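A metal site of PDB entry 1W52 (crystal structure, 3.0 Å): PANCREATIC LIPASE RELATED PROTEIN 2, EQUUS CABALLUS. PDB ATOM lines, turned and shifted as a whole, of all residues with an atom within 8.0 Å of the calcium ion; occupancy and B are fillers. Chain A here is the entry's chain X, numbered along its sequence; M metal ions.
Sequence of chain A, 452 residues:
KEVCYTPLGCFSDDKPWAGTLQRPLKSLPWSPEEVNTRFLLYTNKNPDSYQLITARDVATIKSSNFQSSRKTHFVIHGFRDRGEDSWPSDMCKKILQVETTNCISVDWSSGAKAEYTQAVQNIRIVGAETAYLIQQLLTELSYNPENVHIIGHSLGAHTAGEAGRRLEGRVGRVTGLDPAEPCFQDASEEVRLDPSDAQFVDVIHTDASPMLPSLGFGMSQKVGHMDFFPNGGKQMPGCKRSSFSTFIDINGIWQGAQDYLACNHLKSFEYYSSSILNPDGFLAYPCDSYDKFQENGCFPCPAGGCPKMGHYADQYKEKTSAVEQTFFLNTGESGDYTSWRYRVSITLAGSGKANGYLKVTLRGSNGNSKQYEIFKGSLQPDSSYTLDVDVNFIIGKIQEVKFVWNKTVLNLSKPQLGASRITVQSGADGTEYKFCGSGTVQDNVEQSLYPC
OD2 of Asp 194 sits at hydrogen-bond distance from OG of Ser 196. The backbone carbonyl oxygen (O) of Ala 187 is in hydrogen-bond range of the guanidinium group (NE) of Arg 192.
Merely in contact with the calcium ion: Arg 192. Of the 21 residues printed, 4 come within 4 Å of the calcium ion. The nearest printed residue that does not touch the calcium ion is Leu 193 (4.03 Å).
The calcium ion is bound by the backbone carbonyl oxygen (O) of Glu 189 (2.2 Å), the side-chain carboxylate (OD1) of Asp 194 (2.5 Å), the side-chain carboxylate (OD1) of Asp 197 (2.5 Å) and the side-chain carboxylate (OD2) of Asp 197 (2.5 Å). The calcium ion has four donor atoms within binding distance.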
ATOM      1  N   TRP A  17       0.635  22.410  29.966  1.00  0.00           N
ATOM      2  CA  TRP A  17       1.513  21.297  29.595  1.00  0.00           C
ATOM      3  C   TRP A  17       0.803  20.102  28.994  1.00  0.00           C
ATOM      4  O   TRP A  17       1.447  19.271  28.354  1.00  0.00           O
ATOM      5  CB  TRP A  17       2.356  20.869  30.798  1.00  0.00           C
ATOM      6  CG  TRP A  17       3.055  22.072  31.382  1.00  0.00           C
ATOM      7  CD1 TRP A  17       2.679  22.761  32.490  1.00  0.00           C
ATOM      8  CD2 TRP A  17       4.181  22.764  30.834  1.00  0.00           C
ATOM      9  NE1 TRP A  17       3.530  23.824  32.692  1.00  0.00           N
ATOM     10  CE2 TRP A  17       4.465  23.849  31.696  1.00  0.00           C
ATOM     11  CE3 TRP A  17       5.018  22.553  29.746  1.00  0.00           C
ATOM     12  CZ2 TRP A  17       5.532  24.709  31.494  1.00  0.00           C
ATOM     13  CZ3 TRP A  17       6.049  23.418  29.524  1.00  0.00           C
ATOM     14  CH2 TRP A  17       6.298  24.493  30.382  1.00  0.00           C
ATOM     15  N   HIS A 158      11.975  24.030  20.482  1.00  0.00           N
ATOM     16  CA  HIS A 158      11.124  24.298  21.622  1.00  0.00           C
ATOM     17  C   HIS A 158      11.852  23.988  22.961  1.00  0.00           C
ATOM     18  O   HIS A 158      11.675  24.676  23.987  1.00  0.00           O
ATOM     19  CB  HIS A 158       9.873  23.454  21.490  1.00  0.00           C
ATOM     20  CG  HIS A 158       8.959  23.906  20.412  1.00  0.00           C
ATOM     21  ND1 HIS A 158       8.576  25.225  20.264  1.00  0.00           N
ATOM     22  CD2 HIS A 158       8.352  23.225  19.402  1.00  0.00           C
ATOM     23  CE1 HIS A 158       7.763  25.326  19.227  1.00  0.00           C
ATOM     24  NE2 HIS A 158       7.607  24.137  18.679  1.00  0.00           N
ATOM     25  N   ALA A 160      15.055  24.364  23.482  1.00  0.00           N
ATOM     26  CA  ALA A 160      15.880  25.524  23.687  1.00  0.00           C
ATOM     27  C   ALA A 160      15.014  26.678  24.232  1.00  0.00           C
ATOM     28  O   ALA A 160      15.391  27.328  25.178  1.00  0.00           O
ATOM     29  CB  ALA A 160      16.517  25.927  22.398  1.00  0.00           C
ATOM     30  N   GLY A 161      13.835  26.932  23.670  1.00  0.00           N
ATOM     31  CA  GLY A 161      12.975  27.992  24.159  1.00  0.00           C
ATOM     32  C   GLY A 161      12.551  27.724  25.592  1.00  0.00           C
ATOM     33  O   GLY A 161      12.048  28.628  26.275  1.00  0.00           O
ATOM     34  N   GLU A 162      12.708  26.461  26.030  1.00  0.00           N
ATOM     35  CA  GLU A 162      12.259  26.080  27.350  1.00  0.00           C
ATOM     36  C   GLU A 162      13.306  26.515  28.330  1.00  0.00           C
ATOM     37  O   GLU A 162      12.990  27.364  29.180  1.00  0.00           O
ATOM     38  CB  GLU A 162      11.964  24.575  27.485  1.00  0.00           C
ATOM     39  CG  GLU A 162      11.842  24.085  28.937  1.00  0.00           C
ATOM     40  CD  GLU A 162      10.537  24.471  29.666  1.00  0.00           C
ATOM     41  OE1 GLU A 162       9.880  25.506  29.371  1.00  0.00           O
ATOM     42  OE2 GLU A 162      10.171  23.700  30.602  1.00  0.00           O
ATOM     43  N   GLY A 164      15.469  28.595  27.832  1.00  0.00           N
ATOM     44  CA  GLY A 164      15.496  30.031  27.777  1.00  0.00           C
ATOM     45  C   GLY A 164      14.529  30.728  28.731  1.00  0.00           C
ATOM     46  O   GLY A 164      14.851  31.788  29.308  1.00  0.00           O
ATOM     47  N   ARG A 165      13.347  30.151  28.849  1.00  0.00           N
ATOM     48  CA  ARG A 165      12.307  30.649  29.723  1.00  0.00           C
ATOM     49  C   ARG A 165      12.614  30.348  31.203  1.00  0.00           C
ATOM     50  O   ARG A 165      12.299  31.135  32.099  1.00  0.00           O
ATOM     51  CB  ARG A 165      11.017  30.004  29.335  1.00  0.00           C
ATOM     52  CG  ARG A 165       9.828  30.346  30.192  1.00  0.00           C
ATOM     53  CD  ARG A 165       8.675  29.326  30.061  1.00  0.00           C
ATOM     54  NE  ARG A 165       9.103  28.051  30.602  1.00  0.00           N
ATOM     55  CZ  ARG A 165       8.768  27.587  31.795  1.00  0.00           C
ATOM     56  NH1 ARG A 165       7.952  28.308  32.572  1.00  0.00           N
ATOM     57  NH2 ARG A 165       9.226  26.417  32.233  1.00  0.00           N
ATOM     58  N   ARG A 166      13.240  29.211  31.478  1.00  0.00           N
ATOM     59  CA  ARG A 166      13.668  28.957  32.816  1.00  0.00           C
ATOM     60  C   ARG A 166      14.651  30.022  33.269  1.00  0.00           C
ATOM     61  O   ARG A 166      14.706  30.299  34.428  1.00  0.00           O
ATOM     62  CB  ARG A 166      14.280  27.577  32.942  1.00  0.00           C
ATOM     63  CG  ARG A 166      13.279  26.494  32.573  1.00  0.00           C
ATOM     64  CD  ARG A 166      13.890  25.091  32.428  1.00  0.00           C
ATOM     65  NE  ARG A 166      13.668  24.281  33.623  1.00  0.00           N
ATOM     66  CZ  ARG A 166      12.477  23.895  34.040  1.00  0.00           C
ATOM     67  NH1 ARG A 166      11.384  24.225  33.365  1.00  0.00           N
ATOM     68  NH2 ARG A 166      12.379  23.176  35.150  1.00  0.00           N
ATOM     69  N   ALA A 187      -0.085  27.720  20.985  1.00  0.00           N
ATOM     70  CA  ALA A 187      -0.165  27.298  22.367  1.00  0.00           C
ATOM     71  C   ALA A 187       0.450  28.380  23.298  1.00  0.00           C
ATOM     72  O   ALA A 187       1.046  29.348  22.834  1.00  0.00           O
ATOM     73  CB  ALA A 187       0.480  25.959  22.541  1.00  0.00           C
ATOM     74  N   SER A 188       0.237  28.238  24.604  1.00  0.00           N
ATOM     75  CA  SER A 188       0.828  29.152  25.550  1.00  0.00           C
ATOM     76  C   SER A 188       2.292  29.191  25.230  1.00  0.00           C
ATOM     77  O   SER A 188       2.866  28.176  24.803  1.00  0.00           O
ATOM     78  CB  SER A 188       0.677  28.648  26.970  1.00  0.00           C
ATOM     79  OG  SER A 188       1.104  29.641  27.892  1.00  0.00           O
ATOM     80  N   GLU A 189       2.886  30.361  25.463  1.00  0.00           N
ATOM     81  CA  GLU A 189       4.265  30.605  25.151  1.00  0.00           C
ATOM     82  C   GLU A 189       5.035  29.856  26.203  1.00  0.00           C
ATOM     83  O   GLU A 189       6.205  29.578  26.057  1.00  0.00           O
ATOM     84  CB  GLU A 189       4.530  32.108  25.165  1.00  0.00           C
ATOM     85  CG  GLU A 189       3.546  32.931  24.307  1.00  0.00           C
ATOM     86  CD  GLU A 189       3.828  34.439  24.352  1.00  0.00           C
ATOM     87  OE1 GLU A 189       3.617  35.042  25.418  1.00  0.00           O
ATOM     88  OE2 GLU A 189       4.252  35.043  23.351  1.00  0.00           O
ATOM     89  N   GLU A 190       4.358  29.485  27.271  1.00  0.00           N
ATOM     90  CA  GLU A 190       5.001  28.731  28.323  1.00  0.00           C
ATOM     91  C   GLU A 190       5.578  27.411  27.800  1.00  0.00           C
ATOM     92  O   GLU A 190       6.573  26.871  28.328  1.00  0.00           O
ATOM     93  CB  GLU A 190       4.010  28.532  29.500  1.00  0.00           C
ATOM     94  CG  GLU A 190       4.515  27.583  30.584  1.00  0.00           C
ATOM     95  CD  GLU A 190       3.879  27.763  31.971  1.00  0.00           C
ATOM     96  OE1 GLU A 190       2.705  28.162  32.042  1.00  0.00           O
ATOM     97  OE2 GLU A 190       4.551  27.457  32.991  1.00  0.00           O
ATOM     98  N   VAL A 191       4.956  26.876  26.741  1.00  0.00           N
ATOM     99  CA  VAL A 191       5.219  25.485  26.259  1.00  0.00           C
ATOM    100  C   VAL A 191       5.988  25.451  24.981  1.00  0.00           C
ATOM    101  O   VAL A 191       6.617  24.459  24.654  1.00  0.00           O
ATOM    102  CB  VAL A 191       3.904  24.649  26.059  1.00  0.00           C
ATOM    103  CG1 VAL A 191       3.155  24.546  27.377  1.00  0.00           C
ATOM    104  CG2 VAL A 191       3.015  25.292  25.015  1.00  0.00           C
ATOM    105  N   ARG A 192       5.927  26.544  24.259  1.00  0.00           N
ATOM    106  CA  ARG A 192       6.580  26.630  23.012  1.00  0.00           C
ATOM    107  C   ARG A 192       7.835  27.515  23.102  1.00  0.00           C
ATOM    108  O   ARG A 192       8.646  27.387  24.049  1.00  0.00           O
ATOM    109  CB  ARG A 192       5.560  27.057  21.946  1.00  0.00           C
ATOM    110  CG  ARG A 192       4.941  28.426  22.069  1.00  0.00           C
ATOM    111  CD  ARG A 192       3.985  28.652  20.998  1.00  0.00           C
ATOM    112  NE  ARG A 192       3.383  29.974  20.896  1.00  0.00           N
ATOM    113  CZ  ARG A 192       4.023  31.119  20.635  1.00  0.00           C
ATOM    114  NH1 ARG A 192       5.352  31.171  20.549  1.00  0.00           N
ATOM    115  NH2 ARG A 192       3.342  32.250  20.505  1.00  0.00           N
ATOM    116  N   LEU A 193       8.056  28.284  22.037  1.00  0.00           N
ATOM    117  CA  LEU A 193       9.226  29.077  21.813  1.00  0.00           C
ATOM    118  C   LEU A 193       8.699  30.389  21.233  1.00  0.00           C
ATOM    119  O   LEU A 193       7.919  30.395  20.247  1.00  0.00           O
ATOM    120  CB  LEU A 193      10.189  28.389  20.837  1.00  0.00           C
ATOM    121  CG  LEU A 193      11.100  29.390  20.059  1.00  0.00           C
ATOM    122  CD1 LEU A 193      11.953  30.178  21.019  1.00  0.00           C
ATOM    123  CD2 LEU A 193      12.024  28.810  18.963  1.00  0.00           C
ATOM    124  N   ASP A 194       9.135  31.495  21.818  1.00  0.00           N
ATOM    125  CA  ASP A 194       8.647  32.785  21.419  1.00  0.00           C
ATOM    126  C   ASP A 194       9.742  33.731  21.753  1.00  0.00           C
ATOM    127  O   ASP A 194      10.625  33.340  22.532  1.00  0.00           O
ATOM    128  CB  ASP A 194       7.345  33.128  22.161  1.00  0.00           C
ATOM    129  CG  ASP A 194       7.556  33.480  23.650  1.00  0.00           C
ATOM    130  OD1 ASP A 194       7.734  32.530  24.491  1.00  0.00           O
ATOM    131  OD2 ASP A 194       7.502  34.693  24.043  1.00  0.00           O
ATOM    132  N   PRO A 195       9.662  34.974  21.302  1.00  0.00           N
ATOM    133  CA  PRO A 195      10.780  35.919  21.433  1.00  0.00           C
ATOM    134  C   PRO A 195      11.223  36.213  22.883  1.00  0.00           C
ATOM    135  O   PRO A 195      12.312  36.735  23.153  1.00  0.00           O
ATOM    136  CB  PRO A 195      10.227  37.200  20.777  1.00  0.00           C
ATOM    137  CG  PRO A 195       9.041  36.740  19.853  1.00  0.00           C
ATOM    138  CD  PRO A 195       8.485  35.618  20.688  1.00  0.00           C
ATOM    139  N   SER A 196      10.342  35.913  23.819  1.00  0.00           N
ATOM    140  CA  SER A 196      10.621  36.167  25.216  1.00  0.00           C
ATOM    141  C   SER A 196      11.576  35.144  25.829  1.00  0.00           C
ATOM    142  O   SER A 196      11.922  35.292  26.992  1.00  0.00           O
ATOM    143  CB  SER A 196       9.293  36.172  26.025  1.00  0.00           C
ATOM    144  OG  SER A 196       8.875  34.862  26.444  1.00  0.00           O
ATOM    145  N   ASP A 197      11.982  34.112  25.106  1.00  0.00           N
ATOM    146  CA  ASP A 197      12.752  33.084  25.802  1.00  0.00           C
ATOM    147  C   ASP A 197      14.233  33.433  25.755  1.00  0.00           C
ATOM    148  O   ASP A 197      15.053  32.817  26.446  1.00  0.00           O
ATOM    149  CB  ASP A 197      12.471  31.672  25.220  1.00  0.00           C
ATOM    150  CG  ASP A 197      10.975  31.274  25.307  1.00  0.00           C
ATOM    151  OD1 ASP A 197      10.306  31.426  26.368  1.00  0.00           O
ATOM    152  OD2 ASP A 197      10.386  30.770  24.335  1.00  0.00           O
ATOM    153  N   ALA A 198      14.578  34.420  24.922  1.00  0.00           N
ATOM    154  CA  ALA A 198      15.963  34.898  24.845  1.00  0.00           C
ATOM    155  C   ALA A 198      16.008  36.370  24.511  1.00  0.00           C
ATOM    156  O   ALA A 198      14.997  36.955  24.167  1.00  0.00           O
ATOM    157  CB  ALA A 198      16.757  34.115  23.873  1.00  0.00           C
ATOM    158  N   VAL A 223       7.648  33.194  15.546  1.00  0.00           N
ATOM    159  CA  VAL A 223       7.982  33.065  16.976  1.00  0.00           C
ATOM    160  C   VAL A 223       9.298  33.652  17.395  1.00  0.00           C
ATOM    161  O   VAL A 223       9.803  33.287  18.413  1.00  0.00           O
ATOM    162  CB  VAL A 223       8.041  31.591  17.430  1.00  0.00           C
ATOM    163  CG1 VAL A 223       6.777  30.903  17.075  1.00  0.00           C
ATOM    164  CG2 VAL A 223       9.156  30.900  16.775  1.00  0.00           C
HETATM  165 CA    CA M   1       8.248  30.330  25.517  1.00  0.00          CA
